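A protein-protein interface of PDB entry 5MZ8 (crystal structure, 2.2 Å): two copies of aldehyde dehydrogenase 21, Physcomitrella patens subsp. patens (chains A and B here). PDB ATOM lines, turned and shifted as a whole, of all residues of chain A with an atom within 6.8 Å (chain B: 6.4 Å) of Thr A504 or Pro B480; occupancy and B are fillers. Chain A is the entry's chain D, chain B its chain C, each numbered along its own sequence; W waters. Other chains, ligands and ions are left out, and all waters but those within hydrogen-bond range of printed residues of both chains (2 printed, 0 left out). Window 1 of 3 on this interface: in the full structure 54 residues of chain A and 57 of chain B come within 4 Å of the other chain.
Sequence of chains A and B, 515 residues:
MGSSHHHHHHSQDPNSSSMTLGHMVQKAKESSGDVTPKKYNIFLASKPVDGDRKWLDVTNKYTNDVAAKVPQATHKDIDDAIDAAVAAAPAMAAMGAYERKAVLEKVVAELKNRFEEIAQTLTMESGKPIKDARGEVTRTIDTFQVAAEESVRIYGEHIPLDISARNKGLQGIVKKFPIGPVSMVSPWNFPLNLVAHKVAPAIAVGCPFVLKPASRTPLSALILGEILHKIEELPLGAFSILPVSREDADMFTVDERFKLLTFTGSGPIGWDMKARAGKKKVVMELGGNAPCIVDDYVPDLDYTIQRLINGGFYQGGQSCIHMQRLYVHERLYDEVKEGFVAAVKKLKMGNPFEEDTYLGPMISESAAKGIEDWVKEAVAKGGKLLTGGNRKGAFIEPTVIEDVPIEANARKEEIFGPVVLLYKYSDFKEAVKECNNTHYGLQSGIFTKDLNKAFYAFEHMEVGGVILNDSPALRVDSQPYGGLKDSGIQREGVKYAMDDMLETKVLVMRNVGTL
O of Thr A504 lies within hydrogen-bond range of NH2 of Arg B491, at 2.8 Å.
OE1 of Glu A503 is in salt-bridge range of NH2 of Arg B491 (2.8 Å).
O of Gly B464 lies within hydrogen-bond range of N of Val A506, 3.2 Å away.
The backbone carbonyl oxygen (O) of Phe A177 sits at hydrogen-bond distance from the backbone NH (N) of Glu A503, 2.7 Å away.
N of Val B476 is in hydrogen-bond range of OE1 of Gln B479 (3.0 Å).
The backbone NH of Lys A175 is in hydrogen-bond range of the backbone carbonyl oxygen of Lys A505.
The side-chain amide oxygen of Gln B443 lies within hydrogen-bond range of the side-chain amide nitrogen of Gln B479, at 3.0 Å.
The side-chain amino group of Lys A281 lies within salt-bridge range of the side-chain carboxylate of Glu A503 (3.1 Å).
Val B476 touches Leu A161.
OG of Ser B478 touches CD2 of Leu A161, at 3.8 Å.
Leu A161 touches Gln B479.
CD2 of Leu B484 touches CD of Glu A503, 3.6 Å away.
Gly B464 touches Thr A504.
Thr A504 touches Pro B480.
CG of Lys A505 touches O of Val B463, at 3.4 Å.
Lys A505 touches Gly B464 (CA to O, 3.4 Å).
Val A506 touches Gly B465 (O to CA, 3.3 Å).
CG1 of Val A506 touches O of Pro B480, at 3.7 Å.
Printed residues of chain B within 4 Å of Glu A503: Leu B484 (3.6 Å) and Arg B491 (2.8 Å).
Printed residues of chain B within 4 Å of Thr A504: Gly B464, Pro B480 and Arg B491.
Printed residues of chain B within 4 Å of Val A506: Gly B464, Gly B465 and Pro B480.
Pro B480 touches just these residues of chain A: Thr A504 and Val A506.
Gly B482 touches none of the printed residues of chain A.
Tyr B496 touches none of the printed residues of chain A.
The nearest residue of chain B that does not touch Thr A504 is Val B463 (4.8 Å).
The nearest residue of chain A that does not touch Pro B480 is Val A174 (4.1 Å).
Hydrophobic or aromatic side chains of chain B that line the printed part of chain A: Val B476, Pro B480 and Leu B484.
Along chain A the printed residues that touch a printed residue of chain B span positions 161 to 508.
No position is printed for both chains.
Of the 14 pairs that touch across the chains among the printed residues, none has its exchanged pair printed and touching as well.
Water W2 lies within hydrogen-bond range of O of Thr A504 (2.7 Å), O of Val B463 (3.0 Å) and NH2 of Arg B491 (3.3 Å).
Water W1 lies within hydrogen-bond range of OE2 of Glu A503 and NH1 of Arg B491.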
ATOM      1  N   ILE A 159      15.510  12.908  21.775  1.00  0.00           N
ATOM      2  CA  ILE A 159      16.254  14.147  21.638  1.00  0.00           C
ATOM      3  C   ILE A 159      17.687  14.059  22.192  1.00  0.00           C
ATOM      4  O   ILE A 159      17.891  13.574  23.308  1.00  0.00           O
ATOM      5  CB  ILE A 159      15.483  15.372  22.222  1.00  0.00           C
ATOM      6  CG1 ILE A 159      15.234  15.265  23.764  1.00  0.00           C
ATOM      7  CG2 ILE A 159      14.175  15.618  21.449  1.00  0.00           C
ATOM      8  CD1 ILE A 159      14.811  16.606  24.475  1.00  0.00           C
ATOM      9  N   LEU A 161      20.695  15.566  24.184  1.00  0.00           N
ATOM     10  CA  LEU A 161      20.687  16.643  25.171  1.00  0.00           C
ATOM     11  C   LEU A 161      22.089  17.197  25.452  1.00  0.00           C
ATOM     12  O   LEU A 161      22.227  18.178  26.172  1.00  0.00           O
ATOM     13  CB  LEU A 161      19.935  16.246  26.443  1.00  0.00           C
ATOM     14  CG  LEU A 161      18.395  16.225  26.358  1.00  0.00           C
ATOM     15  CD1 LEU A 161      17.798  15.613  27.621  1.00  0.00           C
ATOM     16  CD2 LEU A 161      17.820  17.628  26.146  1.00  0.00           C
ATOM     17  N   VAL A 174      11.176  12.056  24.905  1.00  0.00           N
ATOM     18  CA  VAL A 174      10.028  12.928  25.155  1.00  0.00           C
ATOM     19  C   VAL A 174       8.784  12.162  24.722  1.00  0.00           C
ATOM     20  O   VAL A 174       8.699  11.725  23.576  1.00  0.00           O
ATOM     21  CB  VAL A 174      10.164  14.294  24.437  1.00  0.00           C
ATOM     22  CG1 VAL A 174       9.035  15.226  24.827  1.00  0.00           C
ATOM     23  CG2 VAL A 174      11.504  14.945  24.744  1.00  0.00           C
ATOM     24  N   LYS A 175       7.867  11.925  25.656  1.00  0.00           N
ATOM     25  CA  LYS A 175       6.640  11.166  25.414  1.00  0.00           C
ATOM     26  C   LYS A 175       5.451  11.961  25.924  1.00  0.00           C
ATOM     27  O   LYS A 175       5.599  12.736  26.875  1.00  0.00           O
ATOM     28  CB  LYS A 175       6.738   9.815  26.138  1.00  0.00           C
ATOM     29  CG  LYS A 175       5.890   8.704  25.576  1.00  0.00           C
ATOM     30  CD  LYS A 175       6.453   7.367  25.993  1.00  0.00           C
ATOM     31  CE  LYS A 175       5.527   6.580  26.888  1.00  0.00           C
ATOM     32  NZ  LYS A 175       6.093   5.239  27.224  1.00  0.00           N
ATOM     33  N   LYS A 176       4.286  11.797  25.281  1.00  0.00           N
ATOM     34  CA  LYS A 176       3.060  12.489  25.661  1.00  0.00           C
ATOM     35  C   LYS A 176       2.128  11.576  26.452  1.00  0.00           C
ATOM     36  O   LYS A 176       1.966  10.409  26.105  1.00  0.00           O
ATOM     37  CB  LYS A 176       2.361  13.091  24.442  1.00  0.00           C
ATOM     38  CG  LYS A 176       3.055  14.337  23.904  1.00  0.00           C
ATOM     39  CD  LYS A 176       2.496  14.707  22.541  1.00  0.00           C
ATOM     40  CE  LYS A 176       3.306  15.758  21.826  1.00  0.00           C
ATOM     41  NZ  LYS A 176       3.947  15.189  20.611  1.00  0.00           N
ATOM     42  N   PHE A 177       1.547  12.102  27.535  1.00  0.00           N
ATOM     43  CA  PHE A 177       0.665  11.353  28.428  1.00  0.00           C
ATOM     44  C   PHE A 177      -0.702  12.023  28.547  1.00  0.00           C
ATOM     45  O   PHE A 177      -0.767  13.257  28.465  1.00  0.00           O
ATOM     46  CB  PHE A 177       1.316  11.226  29.825  1.00  0.00           C
ATOM     47  CG  PHE A 177       2.536  10.340  29.877  1.00  0.00           C
ATOM     48  CD1 PHE A 177       3.779  10.814  29.470  1.00  0.00           C
ATOM     49  CD2 PHE A 177       2.445   9.030  30.334  1.00  0.00           C
ATOM     50  CE1 PHE A 177       4.905   9.978  29.487  1.00  0.00           C
ATOM     51  CE2 PHE A 177       3.575   8.197  30.357  1.00  0.00           C
ATOM     52  CZ  PHE A 177       4.799   8.683  29.944  1.00  0.00           C
ATOM     53  N   LYS A 281      -6.232  23.675  32.820  1.00  0.00           N
ATOM     54  CA  LYS A 281      -6.066  24.222  31.487  1.00  0.00           C
ATOM     55  C   LYS A 281      -7.477  24.451  30.906  1.00  0.00           C
ATOM     56  O   LYS A 281      -8.445  23.812  31.331  1.00  0.00           O
ATOM     57  CB  LYS A 281      -5.225  23.287  30.600  1.00  0.00           C
ATOM     58  CG  LYS A 281      -3.738  23.293  30.959  1.00  0.00           C
ATOM     59  CD  LYS A 281      -2.910  22.515  29.950  1.00  0.00           C
ATOM     60  CE  LYS A 281      -1.455  22.444  30.333  1.00  0.00           C
ATOM     61  NZ  LYS A 281      -0.625  21.829  29.263  1.00  0.00           N
ATOM     62  N   LEU A 502      -3.013  16.274  26.161  1.00  0.00           N
ATOM     63  CA  LEU A 502      -1.759  15.584  26.389  1.00  0.00           C
ATOM     64  C   LEU A 502      -0.779  16.443  27.150  1.00  0.00           C
ATOM     65  O   LEU A 502      -0.772  17.669  27.000  1.00  0.00           O
ATOM     66  CB  LEU A 502      -1.146  15.093  25.054  1.00  0.00           C
ATOM     67  CG  LEU A 502      -1.823  13.868  24.377  1.00  0.00           C
ATOM     68  CD1 LEU A 502      -1.489  13.801  22.902  1.00  0.00           C
ATOM     69  CD2 LEU A 502      -1.438  12.546  25.047  1.00  0.00           C
ATOM     70  N   GLU A 503       0.046  15.794  27.983  1.00  0.00           N
ATOM     71  CA  GLU A 503       1.115  16.421  28.760  1.00  0.00           C
ATOM     72  C   GLU A 503       2.445  15.818  28.370  1.00  0.00           C
ATOM     73  O   GLU A 503       2.570  14.607  28.223  1.00  0.00           O
ATOM     74  CB  GLU A 503       0.880  16.302  30.272  1.00  0.00           C
ATOM     75  CG  GLU A 503      -0.037  17.373  30.831  1.00  0.00           C
ATOM     76  CD  GLU A 503       0.515  18.776  31.038  1.00  0.00           C
ATOM     77  OE1 GLU A 503       1.723  19.023  30.814  1.00  0.00           O
ATOM     78  OE2 GLU A 503      -0.278  19.633  31.477  1.00  0.00           O
ATOM     79  N   THR A 504       3.427  16.681  28.176  1.00  0.00           N
ATOM     80  CA  THR A 504       4.788  16.326  27.800  1.00  0.00           C
ATOM     81  C   THR A 504       5.555  15.849  29.021  1.00  0.00           C
ATOM     82  O   THR A 504       5.485  16.481  30.077  1.00  0.00           O
ATOM     83  CB  THR A 504       5.444  17.546  27.104  1.00  0.00           C
ATOM     84  OG1 THR A 504       4.797  17.747  25.845  1.00  0.00           O
ATOM     85  CG2 THR A 504       6.949  17.388  26.885  1.00  0.00           C
ATOM     86  N   LYS A 505       6.272  14.725  28.878  1.00  0.00           N
ATOM     87  CA  LYS A 505       7.155  14.175  29.909  1.00  0.00           C
ATOM     88  C   LYS A 505       8.446  13.770  29.245  1.00  0.00           C
ATOM     89  O   LYS A 505       8.420  13.097  28.231  1.00  0.00           O
ATOM     90  CB  LYS A 505       6.545  12.977  30.637  1.00  0.00           C
ATOM     91  CG  LYS A 505       7.208  12.718  32.005  1.00  0.00           C
ATOM     92  CD  LYS A 505       6.795  11.371  32.640  1.00  0.00           C
ATOM     93  CE  LYS A 505       5.325  11.340  32.983  1.00  0.00           C
ATOM     94  NZ  LYS A 505       4.909  10.077  33.634  1.00  0.00           N
ATOM     95  N   VAL A 506       9.574  14.157  29.829  1.00  0.00           N
ATOM     96  CA  VAL A 506      10.886  13.804  29.320  1.00  0.00           C
ATOM     97  C   VAL A 506      11.611  12.870  30.308  1.00  0.00           C
ATOM     98  O   VAL A 506      11.604  13.118  31.516  1.00  0.00           O
ATOM     99  CB  VAL A 506      11.737  15.062  28.921  1.00  0.00           C
ATOM    100  CG1 VAL A 506      12.057  15.974  30.123  1.00  0.00           C
ATOM    101  CG2 VAL A 506      13.008  14.683  28.157  1.00  0.00           C
ATOM    102  N   VAL A 508      15.156  12.136  31.115  1.00  0.00           N
ATOM    103  CA  VAL A 508      16.516  12.646  30.879  1.00  0.00           C
ATOM    104  C   VAL A 508      17.465  11.547  31.333  1.00  0.00           C
ATOM    105  O   VAL A 508      17.451  11.163  32.499  1.00  0.00           O
ATOM    106  CB  VAL A 508      16.805  14.027  31.528  1.00  0.00           C
ATOM    107  CG1 VAL A 508      18.246  14.456  31.281  1.00  0.00           C
ATOM    108  CG2 VAL A 508      15.847  15.088  30.997  1.00  0.00           C
ATOM    109  N   GLN B 443       9.844  17.715  38.744  1.00  0.00           N
ATOM    110  CA  GLN B 443      10.835  16.700  38.363  1.00  0.00           C
ATOM    111  C   GLN B 443      11.096  15.675  39.459  1.00  0.00           C
ATOM    112  O   GLN B 443      10.877  15.944  40.631  1.00  0.00           O
ATOM    113  CB  GLN B 443      12.149  17.334  37.899  1.00  0.00           C
ATOM    114  CG  GLN B 443      12.121  17.599  36.417  1.00  0.00           C
ATOM    115  CD  GLN B 443      13.301  18.277  35.806  1.00  0.00           C
ATOM    116  OE1 GLN B 443      13.175  18.806  34.715  1.00  0.00           O
ATOM    117  NE2 GLN B 443      14.484  18.220  36.430  1.00  0.00           N
ATOM    118  N   VAL B 463       5.207  13.832  36.994  1.00  0.00           N
ATOM    119  CA  VAL B 463       6.092  14.998  36.837  1.00  0.00           C
ATOM    120  C   VAL B 463       6.253  15.363  35.364  1.00  0.00           C
ATOM    121  O   VAL B 463       5.842  14.591  34.500  1.00  0.00           O
ATOM    122  CB  VAL B 463       7.486  14.693  37.484  1.00  0.00           C
ATOM    123  CG1 VAL B 463       7.408  14.630  38.999  1.00  0.00           C
ATOM    124  CG2 VAL B 463       8.086  13.401  36.929  1.00  0.00           C
ATOM    125  N   GLY B 464       6.884  16.504  35.095  1.00  0.00           N
ATOM    126  CA  GLY B 464       7.208  16.931  33.737  1.00  0.00           C
ATOM    127  C   GLY B 464       8.519  16.339  33.218  1.00  0.00           C
ATOM    128  O   GLY B 464       8.738  16.280  32.009  1.00  0.00           O
ATOM    129  N   GLY B 465       9.396  15.910  34.129  1.00  0.00           N
ATOM    130  CA  GLY B 465      10.698  15.345  33.807  1.00  0.00           C
ATOM    131  C   GLY B 465      11.181  14.315  34.806  1.00  0.00           C
ATOM    132  O   GLY B 465      11.147  14.563  36.005  1.00  0.00           O
ATOM    133  N   VAL B 476      18.623  20.627  31.193  1.00  0.00           N
ATOM    134  CA  VAL B 476      19.300  21.015  29.956  1.00  0.00           C
ATOM    135  C   VAL B 476      18.420  22.143  29.408  1.00  0.00           C
ATOM    136  O   VAL B 476      17.206  21.984  29.369  1.00  0.00           O
ATOM    137  CB  VAL B 476      19.462  19.843  28.952  1.00  0.00           C
ATOM    138  CG1 VAL B 476      20.203  20.313  27.686  1.00  0.00           C
ATOM    139  CG2 VAL B 476      20.188  18.653  29.600  1.00  0.00           C
ATOM    140  N   SER B 478      17.541  23.141  26.607  1.00  0.00           N
ATOM    141  CA  SER B 478      16.759  22.816  25.407  1.00  0.00           C
ATOM    142  C   SER B 478      15.629  21.816  25.705  1.00  0.00           C
ATOM    143  O   SER B 478      14.744  21.650  24.864  1.00  0.00           O
ATOM    144  CB  SER B 478      17.666  22.279  24.297  1.00  0.00           C
ATOM    145  OG  SER B 478      18.343  21.101  24.708  1.00  0.00           O
ATOM    146  N   GLN B 479      15.659  21.146  26.893  1.00  0.00           N
ATOM    147  CA  GLN B 479      14.648  20.154  27.283  1.00  0.00           C
ATOM    148  C   GLN B 479      13.276  20.776  27.616  1.00  0.00           C
ATOM    149  O   GLN B 479      13.239  21.917  28.082  1.00  0.00           O
ATOM    150  CB  GLN B 479      15.143  19.322  28.489  1.00  0.00           C
ATOM    151  CG  GLN B 479      14.882  19.968  29.851  1.00  0.00           C
ATOM    152  CD  GLN B 479      15.244  19.102  31.014  1.00  0.00           C
ATOM    153  OE1 GLN B 479      16.390  18.687  31.183  1.00  0.00           O
ATOM    154  NE2 GLN B 479      14.281  18.872  31.875  1.00  0.00           N
ATOM    155  N   PRO B 480      12.146  20.030  27.471  1.00  0.00           N
ATOM    156  CA  PRO B 480      10.858  20.588  27.906  1.00  0.00           C
ATOM    157  C   PRO B 480      10.826  20.592  29.431  1.00  0.00           C
ATOM    158  O   PRO B 480      10.964  19.547  30.069  1.00  0.00           O
ATOM    159  CB  PRO B 480       9.828  19.647  27.273  1.00  0.00           C
ATOM    160  CG  PRO B 480      10.543  18.370  27.043  1.00  0.00           C
ATOM    161  CD  PRO B 480      11.996  18.646  26.949  1.00  0.00           C
ATOM    162  N   TYR B 481      10.740  21.784  30.017  1.00  0.00           N
ATOM    163  CA  TYR B 481      10.812  21.956  31.458  1.00  0.00           C
ATOM    164  C   TYR B 481       9.549  22.581  32.016  1.00  0.00           C
ATOM    165  O   TYR B 481       9.129  23.655  31.587  1.00  0.00           O
ATOM    166  CB  TYR B 481      12.073  22.770  31.821  1.00  0.00           C
ATOM    167  CG  TYR B 481      12.183  23.091  33.292  1.00  0.00           C
ATOM    168  CD1 TYR B 481      12.723  22.173  34.185  1.00  0.00           C
ATOM    169  CD2 TYR B 481      11.757  24.320  33.792  1.00  0.00           C
ATOM    170  CE1 TYR B 481      12.836  22.469  35.545  1.00  0.00           C
ATOM    171  CE2 TYR B 481      11.870  24.630  35.146  1.00  0.00           C
ATOM    172  CZ  TYR B 481      12.405  23.698  36.021  1.00  0.00           C
ATOM    173  OH  TYR B 481      12.517  23.993  37.359  1.00  0.00           O
ATOM    174  N   GLY B 482       8.956  21.895  32.980  1.00  0.00           N
ATOM    175  CA  GLY B 482       7.723  22.341  33.609  1.00  0.00           C
ATOM    176  C   GLY B 482       7.095  21.240  34.428  1.00  0.00           C
ATOM    177  O   GLY B 482       7.675  20.155  34.583  1.00  0.00           O
ATOM    178  N   LEU B 484       3.406  19.289  36.489  1.00  0.00           N
ATOM    179  CA  LEU B 484       2.029  18.857  36.649  1.00  0.00           C
ATOM    180  C   LEU B 484       1.587  19.337  38.006  1.00  0.00           C
ATOM    181  O   LEU B 484       2.404  19.862  38.769  1.00  0.00           O
ATOM    182  CB  LEU B 484       1.913  17.319  36.576  1.00  0.00           C
ATOM    183  CG  LEU B 484       2.437  16.635  35.335  1.00  0.00           C
ATOM    184  CD1 LEU B 484       2.172  15.156  35.415  1.00  0.00           C
ATOM    185  CD2 LEU B 484       1.822  17.228  34.063  1.00  0.00           C
ATOM    186  N   ARG B 491       5.321  24.328  29.258  1.00  0.00           N
ATOM    187  CA  ARG B 491       6.758  24.058  29.309  1.00  0.00           C
ATOM    188  C   ARG B 491       7.603  25.214  28.824  1.00  0.00           C
ATOM    189  O   ARG B 491       7.231  25.928  27.892  1.00  0.00           O
ATOM    190  CB  ARG B 491       7.119  22.802  28.459  1.00  0.00           C
ATOM    191  CG  ARG B 491       6.442  21.486  28.865  1.00  0.00           C
ATOM    192  CD  ARG B 491       6.866  20.995  30.245  1.00  0.00           C
ATOM    193  NE  ARG B 491       6.143  19.784  30.623  1.00  0.00           N
ATOM    194  CZ  ARG B 491       4.994  19.769  31.281  1.00  0.00           C
ATOM    195  NH1 ARG B 491       4.417  20.905  31.651  1.00  0.00           N
ATOM    196  NH2 ARG B 491       4.403  18.613  31.568  1.00  0.00           N
ATOM    197  N   GLU B 492       8.760  25.369  29.459  1.00  0.00           N
ATOM    198  CA  GLU B 492       9.845  26.270  29.085  1.00  0.00           C
ATOM    199  C   GLU B 492      10.900  25.341  28.522  1.00  0.00           C
ATOM    200  O   GLU B 492      10.682  24.130  28.465  1.00  0.00           O
ATOM    201  CB  GLU B 492      10.334  27.144  30.240  1.00  0.00           C
ATOM    202  CG  GLU B 492       9.332  28.240  30.562  1.00  0.00           C
ATOM    203  CD  GLU B 492       9.842  29.584  31.049  1.00  0.00           C
ATOM    204  OE1 GLU B 492       9.086  30.563  30.887  1.00  0.00           O
ATOM    205  OE2 GLU B 492      10.973  29.668  31.581  1.00  0.00           O
ATOM    206  N   GLY B 493      11.998  25.899  28.047  1.00  0.00           N
ATOM    207  CA  GLY B 493      12.967  25.168  27.234  1.00  0.00           C
ATOM    208  C   GLY B 493      12.657  25.819  25.913  1.00  0.00           C
ATOM    209  O   GLY B 493      11.486  25.887  25.529  1.00  0.00           O
ATOM    210  N   TYR B 496       9.989  24.939  23.217  1.00  0.00           N
ATOM    211  CA  TYR B 496       8.696  24.753  23.892  1.00  0.00           C
ATOM    212  C   TYR B 496       8.091  26.079  24.340  1.00  0.00           C
ATOM    213  O   TYR B 496       6.882  26.278  24.191  1.00  0.00           O
ATOM    214  CB  TYR B 496       8.830  23.767  25.068  1.00  0.00           C
ATOM    215  CG  TYR B 496       9.508  22.476  24.667  1.00  0.00           C
ATOM    216  CD1 TYR B 496       8.780  21.424  24.119  1.00  0.00           C
ATOM    217  CD2 TYR B 496      10.889  22.329  24.773  1.00  0.00           C
ATOM    218  CE1 TYR B 496       9.408  20.250  23.695  1.00  0.00           C
ATOM    219  CE2 TYR B 496      11.526  21.164  24.346  1.00  0.00           C
ATOM    220  CZ  TYR B 496      10.776  20.115  23.834  1.00  0.00           C
ATOM    221  OH  TYR B 496      11.391  18.949  23.450  1.00  0.00           O
HETATM  222  O   HOH W   1       1.631  21.618  32.619  1.00  0.00           O
HETATM  223  O   HOH W   2       4.148  15.428  32.220  1.00  0.00           O
